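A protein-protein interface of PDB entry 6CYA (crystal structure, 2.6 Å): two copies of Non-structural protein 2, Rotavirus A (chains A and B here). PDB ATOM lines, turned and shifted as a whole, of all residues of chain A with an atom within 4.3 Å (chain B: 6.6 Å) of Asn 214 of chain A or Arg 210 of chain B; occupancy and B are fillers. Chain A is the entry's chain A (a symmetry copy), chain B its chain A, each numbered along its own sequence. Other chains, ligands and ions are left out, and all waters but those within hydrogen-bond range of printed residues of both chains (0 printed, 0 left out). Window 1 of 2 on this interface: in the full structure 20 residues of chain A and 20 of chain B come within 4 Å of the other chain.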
ATOM      1  N   LEU A 209     -24.150  29.035 -22.067  1.00  0.00           N
ATOM      2  CA  LEU A 209     -25.239  28.309 -21.422  1.00  0.00           C
ATOM      3  C   LEU A 209     -24.868  26.848 -21.188  1.00  0.00           C
ATOM      4  O   LEU A 209     -25.244  26.264 -20.166  1.00  0.00           O
ATOM      5  CB  LEU A 209     -26.513  28.412 -22.262  1.00  0.00           C
ATOM      6  CG  LEU A 209     -27.099  29.817 -22.427  1.00  0.00           C
ATOM      7  CD1 LEU A 209     -28.176  29.822 -23.501  1.00  0.00           C
ATOM      8  CD2 LEU A 209     -27.653  30.328 -21.105  1.00  0.00           C
ATOM      9  N   ARG A 210     -24.132  26.241 -22.121  1.00  0.00           N
ATOM     10  CA  ARG A 210     -23.718  24.853 -21.938  1.00  0.00           C
ATOM     11  C   ARG A 210     -22.691  24.722 -20.822  1.00  0.00           C
ATOM     12  O   ARG A 210     -22.712  23.748 -20.062  1.00  0.00           O
ATOM     13  CB  ARG A 210     -23.154  24.294 -23.244  1.00  0.00           C
ATOM     14  CG  ARG A 210     -24.210  23.977 -24.282  1.00  0.00           C
ATOM     15  CD  ARG A 210     -23.587  23.484 -25.574  1.00  0.00           C
ATOM     16  NE  ARG A 210     -24.604  23.118 -26.554  1.00  0.00           N
ATOM     17  CZ  ARG A 210     -24.339  22.725 -27.795  1.00  0.00           C
ATOM     18  NH1 ARG A 210     -23.082  22.641 -28.215  1.00  0.00           N
ATOM     19  NH2 ARG A 210     -25.331  22.415 -28.618  1.00  0.00           N
ATOM     20  N   GLN A 212     -21.688  27.297 -18.275  1.00  0.00           N
ATOM     21  CA  GLN A 212     -22.015  27.928 -17.003  1.00  0.00           C
ATOM     22  C   GLN A 212     -23.384  27.538 -16.457  1.00  0.00           C
ATOM     23  O   GLN A 212     -23.625  27.701 -15.255  1.00  0.00           O
ATOM     24  CB  GLN A 212     -21.942  29.452 -17.154  1.00  0.00           C
ATOM     25  CG  GLN A 212     -21.951  30.224 -15.847  1.00  0.00           C
ATOM     26  CD  GLN A 212     -20.886  29.748 -14.880  1.00  0.00           C
ATOM     27  OE1 GLN A 212     -19.750  29.480 -15.273  1.00  0.00           O
ATOM     28  NE2 GLN A 212     -21.247  29.646 -13.607  1.00  0.00           N
ATOM     29  N   TYR A 213     -24.282  27.025 -17.294  1.00  0.00           N
ATOM     30  CA  TYR A 213     -25.658  26.744 -16.892  1.00  0.00           C
ATOM     31  C   TYR A 213     -26.102  25.378 -17.404  1.00  0.00           C
ATOM     32  O   TYR A 213     -27.208  25.206 -17.920  1.00  0.00           O
ATOM     33  CB  TYR A 213     -26.585  27.851 -17.388  1.00  0.00           C
ATOM     34  CG  TYR A 213     -26.127  29.232 -16.983  1.00  0.00           C
ATOM     35  CD1 TYR A 213     -25.352  30.008 -17.835  1.00  0.00           C
ATOM     36  CD2 TYR A 213     -26.450  29.752 -15.736  1.00  0.00           C
ATOM     37  CE1 TYR A 213     -24.921  31.270 -17.459  1.00  0.00           C
ATOM     38  CE2 TYR A 213     -26.027  31.010 -15.351  1.00  0.00           C
ATOM     39  CZ  TYR A 213     -25.265  31.764 -16.213  1.00  0.00           C
ATOM     40  OH  TYR A 213     -24.845  33.014 -15.827  1.00  0.00           O
ATOM     41  N   ASN A 214     -25.239  24.373 -17.243  1.00  0.00           N
ATOM     42  CA  ASN A 214     -25.525  23.053 -17.791  1.00  0.00           C
ATOM     43  C   ASN A 214     -26.723  22.387 -17.127  1.00  0.00           C
ATOM     44  O   ASN A 214     -27.320  21.482 -17.719  1.00  0.00           O
ATOM     45  CB  ASN A 214     -24.292  22.152 -17.671  1.00  0.00           C
ATOM     46  CG  ASN A 214     -24.112  21.586 -16.273  1.00  0.00           C
ATOM     47  OD1 ASN A 214     -24.098  22.325 -15.285  1.00  0.00           O
ATOM     48  ND2 ASN A 214     -23.967  20.269 -16.183  1.00  0.00           N
ATOM     49  N   LYS A 215     -27.093  22.812 -15.923  1.00  0.00           N
ATOM     50  CA  LYS A 215     -28.233  22.239 -15.224  1.00  0.00           C
ATOM     51  C   LYS A 215     -29.536  22.982 -15.507  1.00  0.00           C
ATOM     52  O   LYS A 215     -30.533  22.743 -14.817  1.00  0.00           O
ATOM     53  CB  LYS A 215     -27.959  22.206 -13.718  1.00  0.00           C
ATOM     54  CG  LYS A 215     -26.951  21.135 -13.297  1.00  0.00           C
ATOM     55  CD  LYS A 215     -26.397  21.398 -11.904  1.00  0.00           C
ATOM     56  CE  LYS A 215     -25.305  22.464 -11.930  1.00  0.00           C
ATOM     57  NZ  LYS A 215     -24.028  21.977 -12.542  1.00  0.00           N
ATOM     58  N   PHE A 216     -29.557  23.859 -16.509  1.00  0.00           N
ATOM     59  CA  PHE A 216     -30.719  24.682 -16.812  1.00  0.00           C
ATOM     60  C   PHE A 216     -31.220  24.399 -18.220  1.00  0.00           C
ATOM     61  O   PHE A 216     -30.427  24.199 -19.146  1.00  0.00           O
ATOM     62  CB  PHE A 216     -30.398  26.173 -16.684  1.00  0.00           C
ATOM     63  CG  PHE A 216     -30.232  26.643 -15.269  1.00  0.00           C
ATOM     64  CD1 PHE A 216     -31.229  27.378 -14.651  1.00  0.00           C
ATOM     65  CD2 PHE A 216     -29.074  26.364 -14.563  1.00  0.00           C
ATOM     66  CE1 PHE A 216     -31.084  27.816 -13.349  1.00  0.00           C
ATOM     67  CE2 PHE A 216     -28.917  26.800 -13.260  1.00  0.00           C
ATOM     68  CZ  PHE A 216     -29.926  27.528 -12.652  1.00  0.00           C
ATOM     69  N   TYR A 231     -34.107  22.327 -14.937  1.00  0.00           N
ATOM     70  CA  TYR A 231     -34.778  21.192 -15.566  1.00  0.00           C
ATOM     71  C   TYR A 231     -35.884  20.632 -14.682  1.00  0.00           C
ATOM     72  O   TYR A 231     -36.907  20.163 -15.194  1.00  0.00           O
ATOM     73  CB  TYR A 231     -33.763  20.099 -15.906  1.00  0.00           C
ATOM     74  CG  TYR A 231     -32.997  20.365 -17.181  1.00  0.00           C
ATOM     75  CD1 TYR A 231     -33.621  20.274 -18.418  1.00  0.00           C
ATOM     76  CD2 TYR A 231     -31.655  20.719 -17.150  1.00  0.00           C
ATOM     77  CE1 TYR A 231     -32.928  20.522 -19.589  1.00  0.00           C
ATOM     78  CE2 TYR A 231     -30.954  20.970 -18.314  1.00  0.00           C
ATOM     79  CZ  TYR A 231     -31.596  20.873 -19.531  1.00  0.00           C
ATOM     80  OH  TYR A 231     -30.905  21.118 -20.696  1.00  0.00           O
ATOM     81  N   LEU B 205     -20.847   7.452 -10.237  1.00  0.00           N
ATOM     82  CA  LEU B 205     -19.931   8.539  -9.911  1.00  0.00           C
ATOM     83  C   LEU B 205     -19.743   9.477 -11.098  1.00  0.00           C
ATOM     84  O   LEU B 205     -19.848  10.702 -10.954  1.00  0.00           O
ATOM     85  CB  LEU B 205     -18.585   7.973  -9.458  1.00  0.00           C
ATOM     86  CG  LEU B 205     -17.572   9.031  -9.015  1.00  0.00           C
ATOM     87  CD1 LEU B 205     -18.094   9.775  -7.793  1.00  0.00           C
ATOM     88  CD2 LEU B 205     -16.219   8.399  -8.730  1.00  0.00           C
ATOM     89  N   VAL B 206     -19.464   8.919 -12.279  1.00  0.00           N
ATOM     90  CA  VAL B 206     -19.188   9.746 -13.452  1.00  0.00           C
ATOM     91  C   VAL B 206     -20.408  10.583 -13.815  1.00  0.00           C
ATOM     92  O   VAL B 206     -20.286  11.760 -14.179  1.00  0.00           O
ATOM     93  CB  VAL B 206     -18.731   8.864 -14.631  1.00  0.00           C
ATOM     94  CG1 VAL B 206     -18.654   9.681 -15.913  1.00  0.00           C
ATOM     95  CG2 VAL B 206     -17.386   8.219 -14.323  1.00  0.00           C
ATOM     96  N   ALA B 207     -21.604   9.997 -13.714  1.00  0.00           N
ATOM     97  CA  ALA B 207     -22.816  10.749 -14.026  1.00  0.00           C
ATOM     98  C   ALA B 207     -22.995  11.925 -13.075  1.00  0.00           C
ATOM     99  O   ALA B 207     -23.429  13.008 -13.487  1.00  0.00           O
ATOM    100  CB  ALA B 207     -24.032   9.826 -13.978  1.00  0.00           C
ATOM    101  N   GLU B 208     -22.656  11.738 -11.799  1.00  0.00           N
ATOM    102  CA  GLU B 208     -22.797  12.830 -10.845  1.00  0.00           C
ATOM    103  C   GLU B 208     -21.740  13.905 -11.082  1.00  0.00           C
ATOM    104  O   GLU B 208     -22.022  15.101 -10.943  1.00  0.00           O
ATOM    105  CB  GLU B 208     -22.727  12.290  -9.414  1.00  0.00           C
ATOM    106  CG  GLU B 208     -22.540  13.361  -8.348  1.00  0.00           C
ATOM    107  CD  GLU B 208     -23.841  14.060  -7.984  1.00  0.00           C
ATOM    108  OE1 GLU B 208     -24.856  13.841  -8.679  1.00  0.00           O
ATOM    109  OE2 GLU B 208     -23.850  14.836  -7.004  1.00  0.00           O
ATOM    110  N   LEU B 209     -20.524  13.505 -11.463  1.00  0.00           N
ATOM    111  CA  LEU B 209     -19.475  14.486 -11.721  1.00  0.00           C
ATOM    112  C   LEU B 209     -19.736  15.247 -13.016  1.00  0.00           C
ATOM    113  O   LEU B 209     -19.457  16.448 -13.102  1.00  0.00           O
ATOM    114  CB  LEU B 209     -18.110  13.799 -11.767  1.00  0.00           C
ATOM    115  CG  LEU B 209     -17.642  13.143 -10.465  1.00  0.00           C
ATOM    116  CD1 LEU B 209     -16.427  12.263 -10.719  1.00  0.00           C
ATOM    117  CD2 LEU B 209     -17.334  14.196  -9.411  1.00  0.00           C
ATOM    118  N   ARG B 210     -20.270  14.570 -14.034  1.00  0.00           N
ATOM    119  CA  ARG B 210     -20.573  15.252 -15.289  1.00  0.00           C
ATOM    120  C   ARG B 210     -21.733  16.225 -15.126  1.00  0.00           C
ATOM    121  O   ARG B 210     -21.728  17.309 -15.719  1.00  0.00           O
ATOM    122  CB  ARG B 210     -20.888  14.231 -16.382  1.00  0.00           C
ATOM    123  CG  ARG B 210     -19.668  13.511 -16.918  1.00  0.00           C
ATOM    124  CD  ARG B 210     -20.050  12.471 -17.955  1.00  0.00           C
ATOM    125  NE  ARG B 210     -18.873  11.820 -18.519  1.00  0.00           N
ATOM    126  CZ  ARG B 210     -18.919  10.820 -19.393  1.00  0.00           C
ATOM    127  NH1 ARG B 210     -20.088  10.352 -19.811  1.00  0.00           N
ATOM    128  NH2 ARG B 210     -17.793  10.287 -19.850  1.00  0.00           N
ATOM    129  N   TRP B 211     -22.731  15.858 -14.324  1.00  0.00           N
ATOM    130  CA  TRP B 211     -23.924  16.687 -14.196  1.00  0.00           C
ATOM    131  C   TRP B 211     -23.738  17.789 -13.158  1.00  0.00           C
ATOM    132  O   TRP B 211     -23.953  18.970 -13.451  1.00  0.00           O
ATOM    133  CB  TRP B 211     -25.121  15.810 -13.835  1.00  0.00           C
ATOM    134  CG  TRP B 211     -26.331  16.578 -13.437  1.00  0.00           C
ATOM    135  CD1 TRP B 211     -26.779  16.802 -12.168  1.00  0.00           C
ATOM    136  CD2 TRP B 211     -27.264  17.219 -14.312  1.00  0.00           C
ATOM    137  NE1 TRP B 211     -27.933  17.550 -12.200  1.00  0.00           N
ATOM    138  CE2 TRP B 211     -28.251  17.820 -13.505  1.00  0.00           C
ATOM    139  CE3 TRP B 211     -27.360  17.349 -15.702  1.00  0.00           C
ATOM    140  CZ2 TRP B 211     -29.319  18.537 -14.041  1.00  0.00           C
ATOM    141  CZ3 TRP B 211     -28.418  18.062 -16.232  1.00  0.00           C
ATOM    142  CH2 TRP B 211     -29.385  18.646 -15.404  1.00  0.00           C
ATOM    143  N   GLN B 212     -23.330  17.423 -11.943  1.00  0.00           N
ATOM    144  CA  GLN B 212     -23.250  18.362 -10.831  1.00  0.00           C
ATOM    145  C   GLN B 212     -21.942  19.145 -10.781  1.00  0.00           C
ATOM    146  O   GLN B 212     -21.894  20.199 -10.135  1.00  0.00           O
ATOM    147  CB  GLN B 212     -23.445  17.608  -9.511  1.00  0.00           C
ATOM    148  CG  GLN B 212     -23.696  18.493  -8.303  1.00  0.00           C
ATOM    149  CD  GLN B 212     -24.839  19.464  -8.517  1.00  0.00           C
ATOM    150  OE1 GLN B 212     -25.877  19.105  -9.076  1.00  0.00           O
ATOM    151  NE2 GLN B 212     -24.657  20.700  -8.069  1.00  0.00           N
ATOM    152  N   TYR B 213     -20.889  18.672 -11.441  1.00  0.00           N
ATOM    153  CA  TYR B 213     -19.565  19.281 -11.345  1.00  0.00           C
ATOM    154  C   TYR B 213     -18.925  19.402 -12.724  1.00  0.00           C
ATOM    155  O   TYR B 213     -17.745  19.104 -12.921  1.00  0.00           O
ATOM    156  CB  TYR B 213     -18.685  18.474 -10.393  1.00  0.00           C
ATOM    157  CG  TYR B 213     -19.325  18.248  -9.044  1.00  0.00           C
ATOM    158  CD1 TYR B 213     -20.040  17.088  -8.776  1.00  0.00           C
ATOM    159  CD2 TYR B 213     -19.236  19.208  -8.045  1.00  0.00           C
ATOM    160  CE1 TYR B 213     -20.638  16.886  -7.542  1.00  0.00           C
ATOM    161  CE2 TYR B 213     -19.827  19.017  -6.810  1.00  0.00           C
ATOM    162  CZ  TYR B 213     -20.525  17.857  -6.563  1.00  0.00           C
ATOM    163  OH  TYR B 213     -21.112  17.670  -5.335  1.00  0.00           O
ATOM    164  N   ASN B 214     -19.703  19.868 -13.703  1.00  0.00           N
ATOM    165  CA  ASN B 214     -19.218  19.923 -15.076  1.00  0.00           C
ATOM    166  C   ASN B 214     -18.070  20.908 -15.256  1.00  0.00           C
ATOM    167  O   ASN B 214     -17.312  20.786 -16.223  1.00  0.00           O
ATOM    168  CB  ASN B 214     -20.364  20.276 -16.028  1.00  0.00           C
ATOM    169  CG  ASN B 214     -20.689  21.760 -16.032  1.00  0.00           C
ATOM    170  OD1 ASN B 214     -20.915  22.364 -14.981  1.00  0.00           O
ATOM    171  ND2 ASN B 214     -20.720  22.355 -17.220  1.00  0.00           N
ATOM    172  N   LYS B 215     -17.919  21.871 -14.352  1.00  0.00           N
ATOM    173  CA  LYS B 215     -16.842  22.845 -14.441  1.00  0.00           C
ATOM    174  C   LYS B 215     -15.588  22.414 -13.686  1.00  0.00           C
ATOM    175  O   LYS B 215     -14.682  23.232 -13.495  1.00  0.00           O
ATOM    176  CB  LYS B 215     -17.325  24.206 -13.932  1.00  0.00           C
ATOM    177  CG  LYS B 215     -18.277  24.923 -14.891  1.00  0.00           C
ATOM    178  CD  LYS B 215     -19.048  26.035 -14.196  1.00  0.00           C
ATOM    179  CE  LYS B 215     -20.221  25.482 -13.390  1.00  0.00           C
ATOM    180  NZ  LYS B 215     -21.345  24.998 -14.253  1.00  0.00           N
ATOM    181  N   ARG B 263     -11.599   5.684 -16.902  1.00  0.00           N
ATOM    182  CA  ARG B 263     -12.942   6.119 -17.266  1.00  0.00           C
ATOM    183  C   ARG B 263     -13.473   7.224 -16.362  1.00  0.00           C
ATOM    184  O   ARG B 263     -14.515   7.813 -16.678  1.00  0.00           O
ATOM    185  CB  ARG B 263     -13.902   4.930 -17.243  1.00  0.00           C
ATOM    186  CG  ARG B 263     -13.453   3.763 -18.102  1.00  0.00           C
ATOM    187  CD  ARG B 263     -14.256   2.516 -17.786  1.00  0.00           C
ATOM    188  NE  ARG B 263     -14.048   2.078 -16.411  1.00  0.00           N
ATOM    189  CZ  ARG B 263     -14.758   1.126 -15.817  1.00  0.00           C
ATOM    190  NH1 ARG B 263     -15.729   0.509 -16.481  1.00  0.00           N
ATOM    191  NH2 ARG B 263     -14.501   0.789 -14.560  1.00  0.00           N
ATOM    192  N   PRO B 299     -16.200   7.592 -22.693  1.00  0.00           N
ATOM    193  CA  PRO B 299     -16.967   6.451 -22.189  1.00  0.00           C
ATOM    194  C   PRO B 299     -18.326   6.869 -21.650  1.00  0.00           C
ATOM    195  O   PRO B 299     -18.550   8.064 -21.445  1.00  0.00           O
ATOM    196  CB  PRO B 299     -16.082   5.917 -21.065  1.00  0.00           C
ATOM    197  CG  PRO B 299     -15.455   7.156 -20.505  1.00  0.00           C
ATOM    198  CD  PRO B 299     -15.255   8.098 -21.680  1.00  0.00           C
ATOM    199  N   PHE B 300     -19.210   5.896 -21.431  1.00  0.00           N
ATOM    200  CA  PHE B 300     -20.498   6.117 -20.776  1.00  0.00           C
ATOM    201  C   PHE B 300     -21.274   7.250 -21.448  1.00  0.00           C
ATOM    202  O   PHE B 300     -21.602   8.268 -20.836  1.00  0.00           O
ATOM    203  CB  PHE B 300     -20.302   6.401 -19.287  1.00  0.00           C
ATOM    204  CG  PHE B 300     -19.446   5.390 -18.578  1.00  0.00           C
ATOM    205  CD1 PHE B 300     -19.594   4.037 -18.828  1.00  0.00           C
ATOM    206  CD2 PHE B 300     -18.493   5.798 -17.656  1.00  0.00           C
ATOM    207  CE1 PHE B 300     -18.807   3.107 -18.173  1.00  0.00           C
ATOM    208  CE2 PHE B 300     -17.704   4.874 -16.997  1.00  0.00           C
ATOM    209  CZ  PHE B 300     -17.859   3.527 -17.256  1.00  0.00           C
ATOM    210  N   LYS B 301     -21.554   7.059 -22.733  1.00  0.00           N
ATOM    211  CA  LYS B 301     -22.277   8.068 -23.492  1.00  0.00           C
ATOM    212  C   LYS B 301     -23.723   8.162 -23.016  1.00  0.00           C
ATOM    213  O   LYS B 301     -24.346   7.166 -22.638  1.00  0.00           O
ATOM    214  CB  LYS B 301     -22.236   7.750 -24.986  1.00  0.00           C
ATOM    215  CG  LYS B 301     -21.184   8.532 -25.759  1.00  0.00           C
ATOM    216  CD  LYS B 301     -19.776   8.206 -25.280  1.00  0.00           C
ATOM    217  CE  LYS B 301     -19.387   6.779 -25.631  1.00  0.00           C
ATOM    218  NZ  LYS B 301     -17.968   6.487 -25.290  1.00  0.00           N
ATOM    219  N   GLY B 302     -24.253   9.383 -23.031  1.00  0.00           N
ATOM    220  CA  GLY B 302     -25.617   9.601 -22.600  1.00  0.00           C
ATOM    221  C   GLY B 302     -25.834   9.557 -21.107  1.00  0.00           C
ATOM    222  O   GLY B 302     -26.986   9.576 -20.665  1.00  0.00           O
ATOM    223  N   LEU B 303     -24.765   9.486 -20.311  1.00  0.00           N
ATOM    224  CA  LEU B 303     -24.928   9.544 -18.862  1.00  0.00           C
ATOM    225  C   LEU B 303     -25.475  10.897 -18.428  1.00  0.00           C
ATOM    226  O   LEU B 303     -26.357  10.973 -17.565  1.00  0.00           O
ATOM    227  CB  LEU B 303     -23.598   9.259 -18.166  1.00  0.00           C
ATOM    228  CG  LEU B 303     -23.529   7.932 -17.412  1.00  0.00           C
ATOM    229  CD1 LEU B 303     -23.831   6.762 -18.336  1.00  0.00           C
ATOM    230  CD2 LEU B 303     -22.178   7.766 -16.741  1.00  0.00           C
ATOM    231  N   SER B 304     -24.962  11.976 -19.020  1.00  0.00           N
ATOM    232  CA  SER B 304     -25.455  13.307 -18.687  1.00  0.00           C
ATOM    233  C   SER B 304     -26.909  13.476 -19.106  1.00  0.00           C
ATOM    234  O   SER B 304     -27.691  14.130 -18.406  1.00  0.00           O
ATOM    235  CB  SER B 304     -24.572  14.364 -19.348  1.00  0.00           C
ATOM    236  OG  SER B 304     -24.536  15.550 -18.575  1.00  0.00           O
ATOM    237  N   LYS B 308     -30.276  14.360 -16.706  1.00  0.00           N
ATOM    238  CA  LYS B 308     -31.089  15.529 -17.026  1.00  0.00           C
ATOM    239  C   LYS B 308     -32.554  15.150 -17.215  1.00  0.00           C
ATOM    240  O   LYS B 308     -33.452  15.859 -16.745  1.00  0.00           O
ATOM    241  CB  LYS B 308     -30.532  16.215 -18.274  1.00  0.00           C
ATOM    242  CG  LYS B 308     -31.549  16.972 -19.105  1.00  0.00           C
ATOM    243  CD  LYS B 308     -30.862  17.670 -20.268  1.00  0.00           C
ATOM    244  CE  LYS B 308     -31.509  17.315 -21.593  1.00  0.00           C
ATOM    245  NZ  LYS B 308     -30.749  17.884 -22.740  1.00  0.00           N
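Of chain B, only Arg 210 (3.7 Å), Trp 211 (3.0 Å), Asn 214 (3.2 Å) and Lys 215 (3.97 Å) come within 4 Å of Asn 214 of chain A. Phe 216 of chain A touches none of the printed residues of chain B. Printed residues of chain A within 4 Å of Trp 211 of chain B: Asn 214, Lys 215 and Tyr 231. Of the printed residues of chain A, Lys 215 of chain B touches Gln 212 (3.7 Å) and Asn 214 (3.97 Å). The nearest residue of chain B that does not touch Asn 214 of chain A is Gln 212 of chain B (5.1 Å). The nearest printed residue of chain A that does not touch Arg 210 of chain B is Lys 215 of chain A (6.1 Å).
O of Leu 209 of chain B lies within hydrogen-bond range of N of Asn 214 of chain B. NH2 of Arg 210 of chain B sits at hydrogen-bond distance from O of Pro 299 of chain B. O of Phe 300 of chain B sits at hydrogen-bond distance from NH1 of Arg 210 of chain B, at 2.8 Å. OD1 of Asn 214 of chain B lies within hydrogen-bond range of NZ of Lys 215 of chain B. O of Leu 209 of chain A sits at hydrogen-bond distance from N of Asn 214 of chain A (3.5 Å). The side-chain amide oxygen of Asn 214 of chain A lies within hydrogen-bond range of the side-chain amino group of Lys 215 of chain A.
Arg 210 of chain A touches Asn 214 of chain B, and with the chains exchanged Asn 214 of chain A touches Arg 210 of chain B. Gln 212 of chain A touches Lys 215 of chain B, and with the chains exchanged Lys 215 of chain A touches Gln 212 of chain B. Asn 214 of chain A touches its own counterpart, Asn 214 of chain B. Asn 214 of chain A touches Lys 215 of chain B, and with the chains exchanged Lys 215 of chain A touches Asn 214 of chain B. Of the 11 pairs that touch across the chains among the printed residues, 7 have their exchanged pair printed and touching as well.
O of Arg 210 of chain A touches ND2 of Asn 214 of chain B (3.7 Å). Gln 212 of chain A touches Lys 215 of chain B. O of Arg 210 of chain B touches ND2 of Asn 214 of chain A, at 3.7 Å. Asn 214 of chain A touches Lys 215 of chain B (OD1 to NZ, 3.97 Å). Gln 212 of chain B touches Lys 215 of chain A (O to NZ, 3.7 Å). Asn 214 of chain B touches Lys 215 of chain A (OD1 to NZ, 3.97 Å). CH2 of Trp 211 of chain B touches CD2 of Tyr 231 of chain A, 3.5 Å away. Lys 308 of chain B touches Tyr 231 of chain A (CD to CZ, 3.4 Å).
The backbone carbonyl oxygen (O) of Trp 211 of chain B lies within hydrogen-bond range of the side-chain amide nitrogen (ND2) of Asn 214 of chain A (3.0 Å). The backbone carbonyl oxygen (O) of Trp 211 of chain B lies within hydrogen-bond range of the side-chain amino group (NZ) of Lys 215 of chain A. The side-chain amide oxygen (OD1) of Asn 214 of chain B lies close to the side-chain amide oxygen (OD1) of Asn 214 of chain A (3.2 Å).
Of the 8 printed residues of chain A, 5 touch a printed residue of chain B. Hydrophobic or aromatic side chains of chain A that line the printed part of chain B: Tyr 231.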
